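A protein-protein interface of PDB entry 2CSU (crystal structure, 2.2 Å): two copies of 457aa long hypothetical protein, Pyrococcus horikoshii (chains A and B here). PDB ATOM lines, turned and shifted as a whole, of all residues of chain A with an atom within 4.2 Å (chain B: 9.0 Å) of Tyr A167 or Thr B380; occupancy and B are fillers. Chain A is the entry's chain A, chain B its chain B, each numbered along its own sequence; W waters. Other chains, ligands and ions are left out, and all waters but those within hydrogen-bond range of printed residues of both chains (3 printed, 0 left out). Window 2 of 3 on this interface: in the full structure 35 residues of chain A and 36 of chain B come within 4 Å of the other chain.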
ATOM      1  N   ILE A 144     -21.737  20.572 -26.063  1.00  0.00           N
ATOM      2  CA  ILE A 144     -20.905  19.789 -26.980  1.00  0.00           C
ATOM      3  C   ILE A 144     -21.808  18.986 -27.918  1.00  0.00           C
ATOM      4  O   ILE A 144     -22.998  18.844 -27.667  1.00  0.00           O
ATOM      5  CB  ILE A 144     -19.943  18.814 -26.224  1.00  0.00           C
ATOM      6  CG1 ILE A 144     -20.738  17.734 -25.497  1.00  0.00           C
ATOM      7  CG2 ILE A 144     -19.061  19.600 -25.243  1.00  0.00           C
ATOM      8  CD1 ILE A 144     -19.845  16.638 -24.910  1.00  0.00           C
ATOM      9  N   THR A 145     -21.256  18.471 -29.008  1.00  0.00           N
ATOM     10  CA  THR A 145     -22.070  17.709 -29.953  1.00  0.00           C
ATOM     11  C   THR A 145     -22.669  16.448 -29.304  1.00  0.00           C
ATOM     12  O   THR A 145     -22.055  15.836 -28.429  1.00  0.00           O
ATOM     13  CB  THR A 145     -21.234  17.325 -31.212  1.00  0.00           C
ATOM     14  OG1 THR A 145     -22.104  16.801 -32.218  1.00  0.00           O
ATOM     15  CG2 THR A 145     -20.203  16.275 -30.873  1.00  0.00           C
ATOM     16  N   ALA A 163     -16.473  14.714 -23.000  1.00  0.00           N
ATOM     17  CA  ALA A 163     -16.503  15.225 -24.366  1.00  0.00           C
ATOM     18  C   ALA A 163     -15.588  14.436 -25.307  1.00  0.00           C
ATOM     19  O   ALA A 163     -15.978  14.073 -26.424  1.00  0.00           O
ATOM     20  CB  ALA A 163     -16.109  16.694 -24.377  1.00  0.00           C
ATOM     21  N   GLY A 164     -14.367  14.174 -24.852  1.00  0.00           N
ATOM     22  CA  GLY A 164     -13.418  13.452 -25.672  1.00  0.00           C
ATOM     23  C   GLY A 164     -13.879  12.053 -26.037  1.00  0.00           C
ATOM     24  O   GLY A 164     -13.585  11.557 -27.122  1.00  0.00           O
ATOM     25  N   ILE A 165     -14.589  11.412 -25.123  1.00  0.00           N
ATOM     26  CA  ILE A 165     -15.089  10.073 -25.359  1.00  0.00           C
ATOM     27  C   ILE A 165     -16.261  10.159 -26.342  1.00  0.00           C
ATOM     28  O   ILE A 165     -16.371   9.349 -27.248  1.00  0.00           O
ATOM     29  CB  ILE A 165     -15.473   9.392 -23.999  1.00  0.00           C
ATOM     30  CG1 ILE A 165     -14.184   8.976 -23.281  1.00  0.00           C
ATOM     31  CG2 ILE A 165     -16.353   8.167 -24.218  1.00  0.00           C
ATOM     32  CD1 ILE A 165     -14.374   8.422 -21.876  1.00  0.00           C
ATOM     33  N   VAL A 166     -17.113  11.166 -26.184  1.00  0.00           N
ATOM     34  CA  VAL A 166     -18.228  11.343 -27.105  1.00  0.00           C
ATOM     35  C   VAL A 166     -17.674  11.469 -28.526  1.00  0.00           C
ATOM     36  O   VAL A 166     -18.151  10.800 -29.446  1.00  0.00           O
ATOM     37  CB  VAL A 166     -19.054  12.592 -26.734  1.00  0.00           C
ATOM     38  CG1 VAL A 166     -20.035  12.941 -27.841  1.00  0.00           C
ATOM     39  CG2 VAL A 166     -19.816  12.334 -25.444  1.00  0.00           C
ATOM     40  N   TYR A 167     -16.651  12.297 -28.713  1.00  0.00           N
ATOM     41  CA  TYR A 167     -16.063  12.457 -30.043  1.00  0.00           C
ATOM     42  C   TYR A 167     -15.463  11.150 -30.499  1.00  0.00           C
ATOM     43  O   TYR A 167     -15.515  10.810 -31.680  1.00  0.00           O
ATOM     44  CB  TYR A 167     -14.963  13.527 -30.061  1.00  0.00           C
ATOM     45  CG  TYR A 167     -15.385  14.849 -29.467  1.00  0.00           C
ATOM     46  CD1 TYR A 167     -16.729  15.221 -29.440  1.00  0.00           C
ATOM     47  CD2 TYR A 167     -14.442  15.726 -28.920  1.00  0.00           C
ATOM     48  CE1 TYR A 167     -17.132  16.424 -28.881  1.00  0.00           C
ATOM     49  CE2 TYR A 167     -14.842  16.940 -28.359  1.00  0.00           C
ATOM     50  CZ  TYR A 167     -16.187  17.275 -28.345  1.00  0.00           C
ATOM     51  OH  TYR A 167     -16.598  18.454 -27.783  1.00  0.00           O
ATOM     52  N   LYS A 168     -14.875  10.419 -29.557  1.00  0.00           N
ATOM     53  CA  LYS A 168     -14.262   9.145 -29.874  1.00  0.00           C
ATOM     54  C   LYS A 168     -15.285   8.176 -30.432  1.00  0.00           C
ATOM     55  O   LYS A 168     -15.131   7.669 -31.538  1.00  0.00           O
ATOM     56  CB  LYS A 168     -13.621   8.536 -28.627  1.00  0.00           C
ATOM     57  CG  LYS A 168     -12.892   7.211 -28.893  1.00  0.00           C
ATOM     58  CD  LYS A 168     -12.210   6.690 -27.631  1.00  0.00           C
ATOM     59  CE  LYS A 168     -11.089   5.710 -27.952  1.00  0.00           C
ATOM     60  NZ  LYS A 168     -11.514   4.425 -28.554  1.00  0.00           N
ATOM     61  N   THR A 169     -16.330   7.918 -29.651  1.00  0.00           N
ATOM     62  CA  THR A 169     -17.395   6.994 -30.035  1.00  0.00           C
ATOM     63  C   THR A 169     -18.105   7.362 -31.336  1.00  0.00           C
ATOM     64  O   THR A 169     -18.493   6.486 -32.104  1.00  0.00           O
ATOM     65  CB  THR A 169     -18.447   6.900 -28.926  1.00  0.00           C
ATOM     66  OG1 THR A 169     -18.801   8.223 -28.503  1.00  0.00           O
ATOM     67  CG2 THR A 169     -17.895   6.111 -27.737  1.00  0.00           C
ATOM     68  N   ILE A 170     -18.277   8.658 -31.570  1.00  0.00           N
ATOM     69  CA  ILE A 170     -18.939   9.148 -32.766  1.00  0.00           C
ATOM     70  C   ILE A 170     -18.217   8.616 -33.988  1.00  0.00           C
ATOM     71  O   ILE A 170     -18.832   8.005 -34.869  1.00  0.00           O
ATOM     72  CB  ILE A 170     -18.963  10.693 -32.788  1.00  0.00           C
ATOM     73  CG1 ILE A 170     -20.005  11.194 -31.783  1.00  0.00           C
ATOM     74  CG2 ILE A 170     -19.276  11.210 -34.199  1.00  0.00           C
ATOM     75  CD1 ILE A 170     -20.059  12.689 -31.616  1.00  0.00           C
ATOM     76  N   LYS A 171     -16.909   8.839 -34.041  1.00  0.00           N
ATOM     77  CA  LYS A 171     -16.124   8.357 -35.164  1.00  0.00           C
ATOM     78  C   LYS A 171     -16.068   6.828 -35.216  1.00  0.00           C
ATOM     79  O   LYS A 171     -16.015   6.242 -36.303  1.00  0.00           O
ATOM     80  CB  LYS A 171     -14.695   8.902 -35.095  1.00  0.00           C
ATOM     81  CG  LYS A 171     -13.801   8.336 -36.182  1.00  0.00           C
ATOM     82  CD  LYS A 171     -12.491   9.092 -36.308  1.00  0.00           C
ATOM     83  CE  LYS A 171     -11.486   8.294 -37.132  1.00  0.00           C
ATOM     84  NZ  LYS A 171     -10.281   9.107 -37.460  1.00  0.00           N
ATOM     85  N   ASN B 301      -5.165  20.512 -21.333  1.00  0.00           N
ATOM     86  CA  ASN B 301      -6.249  21.454 -21.132  1.00  0.00           C
ATOM     87  C   ASN B 301      -7.372  20.699 -20.430  1.00  0.00           C
ATOM     88  O   ASN B 301      -8.477  21.213 -20.300  1.00  0.00           O
ATOM     89  CB  ASN B 301      -6.736  22.022 -22.476  1.00  0.00           C
ATOM     90  CG  ASN B 301      -7.456  20.999 -23.322  1.00  0.00           C
ATOM     91  OD1 ASN B 301      -7.268  19.795 -23.159  1.00  0.00           O
ATOM     92  ND2 ASN B 301      -8.283  21.474 -24.250  1.00  0.00           N
ATOM     93  N   ALA B 349      -9.778  24.395 -19.410  1.00  0.00           N
ATOM     94  CA  ALA B 349     -10.340  24.091 -20.721  1.00  0.00           C
ATOM     95  C   ALA B 349     -10.333  25.327 -21.620  1.00  0.00           C
ATOM     96  O   ALA B 349     -10.630  25.261 -22.805  1.00  0.00           O
ATOM     97  CB  ALA B 349     -11.773  23.584 -20.522  1.00  0.00           C
ATOM     98  N   CYS B 376      -4.498  17.461 -25.252  1.00  0.00           N
ATOM     99  CA  CYS B 376      -5.499  18.461 -25.550  1.00  0.00           C
ATOM    100  C   CYS B 376      -6.802  17.812 -25.992  1.00  0.00           C
ATOM    101  O   CYS B 376      -6.867  17.060 -26.953  1.00  0.00           O
ATOM    102  CB  CYS B 376      -4.969  19.353 -26.671  1.00  0.00           C
ATOM    103  SG  CYS B 376      -6.291  20.211 -27.553  1.00  0.00           S
ATOM    104  N   VAL B 377      -7.845  18.086 -25.207  1.00  0.00           N
ATOM    105  CA  VAL B 377      -9.175  17.871 -25.729  1.00  0.00           C
ATOM    106  C   VAL B 377      -9.585  19.075 -26.581  1.00  0.00           C
ATOM    107  O   VAL B 377      -9.711  20.197 -26.109  1.00  0.00           O
ATOM    108  CB  VAL B 377     -10.111  17.656 -24.544  1.00  0.00           C
ATOM    109  CG1 VAL B 377     -11.499  17.288 -25.054  1.00  0.00           C
ATOM    110  CG2 VAL B 377      -9.569  16.514 -23.690  1.00  0.00           C
ATOM    111  N   VAL B 378      -9.706  18.823 -27.899  1.00  0.00           N
ATOM    112  CA  VAL B 378     -10.011  19.921 -28.807  1.00  0.00           C
ATOM    113  C   VAL B 378     -11.371  20.541 -28.495  1.00  0.00           C
ATOM    114  O   VAL B 378     -12.415  19.913 -28.600  1.00  0.00           O
ATOM    115  CB  VAL B 378      -9.981  19.382 -30.234  1.00  0.00           C
ATOM    116  CG1 VAL B 378     -10.347  20.492 -31.213  1.00  0.00           C
ATOM    117  CG2 VAL B 378      -8.594  18.866 -30.559  1.00  0.00           C
ATOM    118  N   PRO B 379     -11.337  21.809 -28.059  1.00  0.00           N
ATOM    119  CA  PRO B 379     -12.556  22.518 -27.715  1.00  0.00           C
ATOM    120  C   PRO B 379     -13.286  22.993 -28.976  1.00  0.00           C
ATOM    121  O   PRO B 379     -12.694  23.233 -30.020  1.00  0.00           O
ATOM    122  CB  PRO B 379     -12.166  23.713 -26.857  1.00  0.00           C
ATOM    123  CG  PRO B 379     -10.668  23.961 -27.030  1.00  0.00           C
ATOM    124  CD  PRO B 379     -10.188  22.683 -27.870  1.00  0.00           C
ATOM    125  N   THR B 380     -14.619  23.092 -28.848  1.00  0.00           N
ATOM    126  CA  THR B 380     -15.410  23.607 -29.956  1.00  0.00           C
ATOM    127  C   THR B 380     -16.331  24.738 -29.498  1.00  0.00           C
ATOM    128  O   THR B 380     -17.515  24.772 -29.806  1.00  0.00           O
ATOM    129  CB  THR B 380     -16.238  22.461 -30.536  1.00  0.00           C
ATOM    130  OG1 THR B 380     -17.139  21.987 -29.534  1.00  0.00           O
ATOM    131  CG2 THR B 380     -15.319  21.311 -30.962  1.00  0.00           C
ATOM    132  N   PHE B 381     -15.745  25.591 -28.670  1.00  0.00           N
ATOM    133  CA  PHE B 381     -16.485  26.666 -28.043  1.00  0.00           C
ATOM    134  C   PHE B 381     -15.561  27.827 -27.718  1.00  0.00           C
ATOM    135  O   PHE B 381     -14.339  27.690 -27.770  1.00  0.00           O
ATOM    136  CB  PHE B 381     -17.158  26.146 -26.770  1.00  0.00           C
ATOM    137  CG  PHE B 381     -16.230  25.395 -25.845  1.00  0.00           C
ATOM    138  CD1 PHE B 381     -15.319  26.077 -25.040  1.00  0.00           C
ATOM    139  CD2 PHE B 381     -16.272  24.001 -25.775  1.00  0.00           C
ATOM    140  CE1 PHE B 381     -14.468  25.383 -24.175  1.00  0.00           C
ATOM    141  CE2 PHE B 381     -15.425  23.299 -24.914  1.00  0.00           C
ATOM    142  CZ  PHE B 381     -14.521  23.993 -24.111  1.00  0.00           C
ATOM    143  N   ALA B 382     -16.155  28.971 -27.397  1.00  0.00           N
ATOM    144  CA  ALA B 382     -15.405  30.168 -27.050  1.00  0.00           C
ATOM    145  C   ALA B 382     -14.556  30.746 -28.183  1.00  0.00           C
ATOM    146  O   ALA B 382     -13.590  31.469 -27.920  1.00  0.00           O
ATOM    147  CB  ALA B 382     -14.528  29.891 -25.836  1.00  0.00           C
ATOM    148  N   GLY B 383     -14.910  30.435 -29.431  1.00  0.00           N
ATOM    149  CA  GLY B 383     -14.169  30.965 -30.569  1.00  0.00           C
ATOM    150  C   GLY B 383     -12.851  30.293 -30.948  1.00  0.00           C
ATOM    151  O   GLY B 383     -12.215  30.680 -31.939  1.00  0.00           O
ATOM    152  N   MET B 384     -12.423  29.302 -30.171  1.00  0.00           N
ATOM    153  CA  MET B 384     -11.179  28.599 -30.460  1.00  0.00           C
ATOM    154  C   MET B 384     -11.310  27.721 -31.711  1.00  0.00           C
ATOM    155  O   MET B 384     -12.363  27.150 -31.971  1.00  0.00           O
ATOM    156  CB  MET B 384     -10.761  27.747 -29.248  1.00  0.00           C
ATOM    157  CG  MET B 384     -10.218  28.571 -28.062  1.00  0.00           C
ATOM    158  SD  MET B 384     -10.003  27.682 -26.523  1.00  0.00           S
ATOM    159  CE  MET B 384     -11.540  27.914 -25.773  1.00  0.00           C
ATOM    160  N   THR B 385     -10.240  27.636 -32.496  1.00  0.00           N
ATOM    161  CA  THR B 385     -10.244  26.823 -33.703  1.00  0.00           C
ATOM    162  C   THR B 385      -9.857  25.388 -33.361  1.00  0.00           C
ATOM    163  O   THR B 385      -9.422  25.099 -32.245  1.00  0.00           O
ATOM    164  CB  THR B 385      -9.243  27.349 -34.749  1.00  0.00           C
ATOM    165  OG1 THR B 385      -7.908  27.152 -34.269  1.00  0.00           O
ATOM    166  CG2 THR B 385      -9.475  28.836 -35.016  1.00  0.00           C
ATOM    167  N   LEU B 386      -9.999  24.500 -34.339  1.00  0.00           N
ATOM    168  CA  LEU B 386      -9.685  23.090 -34.159  1.00  0.00           C
ATOM    169  C   LEU B 386      -8.184  22.784 -34.190  1.00  0.00           C
ATOM    170  O   LEU B 386      -7.755  21.731 -33.715  1.00  0.00           O
ATOM    171  CB  LEU B 386     -10.400  22.266 -35.244  1.00  0.00           C
ATOM    172  CG  LEU B 386     -11.931  22.368 -35.330  1.00  0.00           C
ATOM    173  CD1 LEU B 386     -12.448  21.637 -36.550  1.00  0.00           C
ATOM    174  CD2 LEU B 386     -12.548  21.795 -34.082  1.00  0.00           C
ATOM    175  N   HIS B 389      -4.489  24.913 -30.831  1.00  0.00           N
ATOM    176  CA  HIS B 389      -3.639  24.323 -29.798  1.00  0.00           C
ATOM    177  C   HIS B 389      -2.449  23.558 -30.393  1.00  0.00           C
ATOM    178  O   HIS B 389      -1.328  23.623 -29.905  1.00  0.00           O
ATOM    179  CB  HIS B 389      -4.500  23.380 -28.957  1.00  0.00           C
ATOM    180  CG  HIS B 389      -5.849  24.008 -28.722  1.00  0.00           C
ATOM    181  ND1 HIS B 389      -6.870  23.935 -29.612  1.00  0.00           N
ATOM    182  CD2 HIS B 389      -6.270  24.766 -27.624  1.00  0.00           C
ATOM    183  CE1 HIS B 389      -7.882  24.633 -29.060  1.00  0.00           C
ATOM    184  NE2 HIS B 389      -7.551  25.142 -27.871  1.00  0.00           N
ATOM    185  N   PHE B 410      -4.138  14.323 -28.723  1.00  0.00           N
ATOM    186  CA  PHE B 410      -5.363  15.090 -28.935  1.00  0.00           C
ATOM    187  C   PHE B 410      -6.608  14.203 -29.049  1.00  0.00           C
ATOM    188  O   PHE B 410      -6.719  13.336 -29.907  1.00  0.00           O
ATOM    189  CB  PHE B 410      -5.200  15.890 -30.226  1.00  0.00           C
ATOM    190  CG  PHE B 410      -4.392  17.127 -29.971  1.00  0.00           C
ATOM    191  CD1 PHE B 410      -3.272  17.058 -29.150  1.00  0.00           C
ATOM    192  CD2 PHE B 410      -4.713  18.305 -30.622  1.00  0.00           C
ATOM    193  CE1 PHE B 410      -2.461  18.174 -28.999  1.00  0.00           C
ATOM    194  CE2 PHE B 410      -3.893  19.420 -30.467  1.00  0.00           C
ATOM    195  CZ  PHE B 410      -2.765  19.358 -29.660  1.00  0.00           C
ATOM    196  N   MET B 411      -7.550  14.415 -28.107  1.00  0.00           N
ATOM    197  CA  MET B 411      -8.911  13.944 -28.334  1.00  0.00           C
ATOM    198  C   MET B 411      -9.713  15.048 -29.025  1.00  0.00           C
ATOM    199  O   MET B 411      -9.545  16.228 -28.764  1.00  0.00           O
ATOM    200  CB  MET B 411      -9.562  13.643 -26.983  1.00  0.00           C
ATOM    201  CG  MET B 411      -8.894  12.508 -26.205  1.00  0.00           C
ATOM    202  SD  MET B 411      -9.454  12.489 -24.492  1.00  0.00           S
ATOM    203  CE  MET B 411      -9.032  10.785 -24.096  1.00  0.00           C
ATOM    204  N   ALA B 412     -10.577  14.646 -29.965  1.00  0.00           N
ATOM    205  CA  ALA B 412     -10.737  13.242 -30.318  1.00  0.00           C
ATOM    206  C   ALA B 412     -11.653  13.087 -31.533  1.00  0.00           C
ATOM    207  O   ALA B 412     -12.253  14.038 -32.019  1.00  0.00           O
ATOM    208  CB  ALA B 412     -11.333  12.516 -29.109  1.00  0.00           C
ATOM    209  N   GLY B 413     -11.718  11.847 -32.060  1.00  0.00           N
ATOM    210  CA  GLY B 413     -12.616  11.588 -33.182  1.00  0.00           C
ATOM    211  C   GLY B 413     -12.310  12.498 -34.371  1.00  0.00           C
ATOM    212  O   GLY B 413     -11.166  12.771 -34.700  1.00  0.00           O
ATOM    213  N   TYR B 414     -13.385  12.942 -35.058  1.00  0.00           N
ATOM    214  CA  TYR B 414     -13.184  13.854 -36.175  1.00  0.00           C
ATOM    215  C   TYR B 414     -12.737  15.233 -35.693  1.00  0.00           C
ATOM    216  O   TYR B 414     -12.122  15.995 -36.427  1.00  0.00           O
ATOM    217  CB  TYR B 414     -14.492  13.992 -36.951  1.00  0.00           C
ATOM    218  CG  TYR B 414     -14.988  12.665 -37.399  1.00  0.00           C
ATOM    219  CD1 TYR B 414     -14.253  11.912 -38.312  1.00  0.00           C
ATOM    220  CD2 TYR B 414     -16.240  12.219 -36.987  1.00  0.00           C
ATOM    221  CE1 TYR B 414     -14.764  10.718 -38.798  1.00  0.00           C
ATOM    222  CE2 TYR B 414     -16.757  11.035 -37.480  1.00  0.00           C
ATOM    223  CZ  TYR B 414     -16.026  10.283 -38.381  1.00  0.00           C
ATOM    224  OH  TYR B 414     -16.503   9.060 -38.811  1.00  0.00           O
ATOM    225  N   VAL B 415     -13.112  15.540 -34.439  1.00  0.00           N
ATOM    226  CA  VAL B 415     -12.800  16.862 -33.915  1.00  0.00           C
ATOM    227  C   VAL B 415     -11.294  17.120 -33.885  1.00  0.00           C
ATOM    228  O   VAL B 415     -10.825  18.237 -34.061  1.00  0.00           O
ATOM    229  CB  VAL B 415     -13.374  16.974 -32.503  1.00  0.00           C
ATOM    230  CG1 VAL B 415     -13.055  18.348 -31.928  1.00  0.00           C
ATOM    231  CG2 VAL B 415     -14.881  16.791 -32.541  1.00  0.00           C
ATOM    232  N   SER B 416     -10.498  16.080 -33.573  1.00  0.00           N
ATOM    233  CA  SER B 416      -9.060  16.310 -33.410  1.00  0.00           C
ATOM    234  C   SER B 416      -8.268  15.948 -34.670  1.00  0.00           C
ATOM    235  O   SER B 416      -7.087  16.238 -34.802  1.00  0.00           O
ATOM    236  CB  SER B 416      -8.566  15.488 -32.224  1.00  0.00           C
ATOM    237  OG  SER B 416      -8.497  14.124 -32.624  1.00  0.00           O
ATOM    238  N   GLU B 417      -8.887  15.340 -35.674  1.00  0.00           N
ATOM    239  CA  GLU B 417      -8.152  14.964 -36.880  1.00  0.00           C
ATOM    240  C   GLU B 417      -7.319  16.060 -37.544  1.00  0.00           C
ATOM    241  O   GLU B 417      -6.166  15.827 -37.894  1.00  0.00           O
ATOM    242  CB  GLU B 417      -9.097  14.344 -37.908  1.00  0.00           C
ATOM    243  CG  GLU B 417      -9.030  12.826 -37.935  1.00  0.00           C
ATOM    244  CD  GLU B 417      -9.923  12.224 -38.999  1.00  0.00           C
ATOM    245  OE1 GLU B 417      -9.875  12.702 -40.153  1.00  0.00           O
ATOM    246  OE2 GLU B 417     -10.668  11.270 -38.679  1.00  0.00           O
ATOM    247  N   GLU B 432      -4.381   9.134 -29.530  1.00  0.00           N
ATOM    248  CA  GLU B 432      -5.747   9.379 -29.083  1.00  0.00           C
ATOM    249  C   GLU B 432      -6.057   8.613 -27.799  1.00  0.00           C
ATOM    250  O   GLU B 432      -7.127   8.760 -27.213  1.00  0.00           O
ATOM    251  CB  GLU B 432      -6.716   8.989 -30.221  1.00  0.00           C
ATOM    252  CG  GLU B 432      -8.217   9.122 -29.934  1.00  0.00           C
ATOM    253  CD  GLU B 432      -9.061   9.225 -31.225  1.00  0.00           C
ATOM    254  OE1 GLU B 432     -10.259   8.867 -31.202  1.00  0.00           O
ATOM    255  OE2 GLU B 432      -8.517   9.679 -32.260  1.00  0.00           O
HETATM  256  O   HOH W   1     -15.852  12.968 -33.682  1.00  0.00           O
HETATM  257  O   HOH W   2     -14.546  20.220 -26.860  1.00  0.00           O
HETATM  258  O   HOH W   3     -18.544  19.601 -29.603  1.00  0.00           O
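Printed residues of chain A that touch a printed residue of chain B: Gly A164, Tyr A167, Lys A168 and Lys A171.
Among the printed residues, 10 pairs touch across the chains.
Among the printed residues, merely in contact across the chains: Gly A164 with Ala B412 (3.2 Å), Tyr A167 with Val B378 (3.8 Å), Tyr A167 with Thr B380 (3.98 Å), Tyr A167 with Ala B412 (3.4 Å), Tyr A167 with Gly B413 (3.4 Å), Tyr A167 with Val B415 (3.7 Å), Lys A168 with Glu B432 (3.9 Å), Lys A171 with Gly B413 (3.9 Å) and Lys A171 with Tyr B414 (3.6 Å).
The side-chain carboxylate of Glu B417 lies within salt-bridge range of the side-chain amino group of Lys A171 (2.5 Å).
SG of Cys B376 sits close to N of Val B378, at 3.7 Å.
O of Met B411 lies within hydrogen-bond range of N of Val B378, 2.7 Å away.
The backbone NH (N) of Ala B412 sits close to the side-chain hydroxyl (OG) of Ser B416 (3.4 Å).
The side-chain carboxylate (OE1) of Glu B432 sits at hydrogen-bond distance from the backbone NH (N) of Gly B413, 3.4 Å away.
Water W2 lies within hydrogen-bond range of O of Val B378 (2.8 Å), OH of Tyr A167 (2.9 Å) and N of Thr B380 (3.5 Å).
Water W3 lies within hydrogen-bond range of OG1 of Thr B380 (2.8 Å), OH of Tyr A167 (2.9 Å) and N of Thr A145 (3.0 Å).
Water W1 lies within hydrogen-bond range of N of Tyr B414 (2.8 Å) and O of Tyr A167 (3.0 Å).
Of chain B, only Ala B412 (3.2 Å) comes within 4 Å of Gly A164.
No residue of chain B comes within 4 Å of Val A166.
Of the printed residues of chain B, Tyr A167 touches Val B378 (3.8 Å), Thr B380 (3.98 Å), Ala B412 (3.4 Å), Gly B413 (3.4 Å) and Val B415 (3.7 Å).
Of the printed residues of chain A, Val B378 touches Tyr A167.
Of the printed residues of chain A, Ala B412 touches Gly A164 (3.2 Å) and Tyr A167 (3.4 Å).
Of the printed residues of chain A, Tyr B414 touches Lys A171.
Of the printed residues of chain A, Val B415 touches Tyr A167.
Printed residues of chain A within 4 Å of Glu B432: Lys A168 (3.9 Å).
The nearest printed residue of chain B that does not touch Tyr A167 is Tyr B414 (4.5 Å).
The nearest printed residue of chain A that does not touch Thr B380 is Ile A144 (5.1 Å).
The nearest printed residue of chain B that does not touch Lys A168 is Ala B412 (4.1 Å).
No position is printed for both chains.
Of the 10 pairs that touch across the chains among the printed residues, none has its exchanged pair printed and touching as well.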
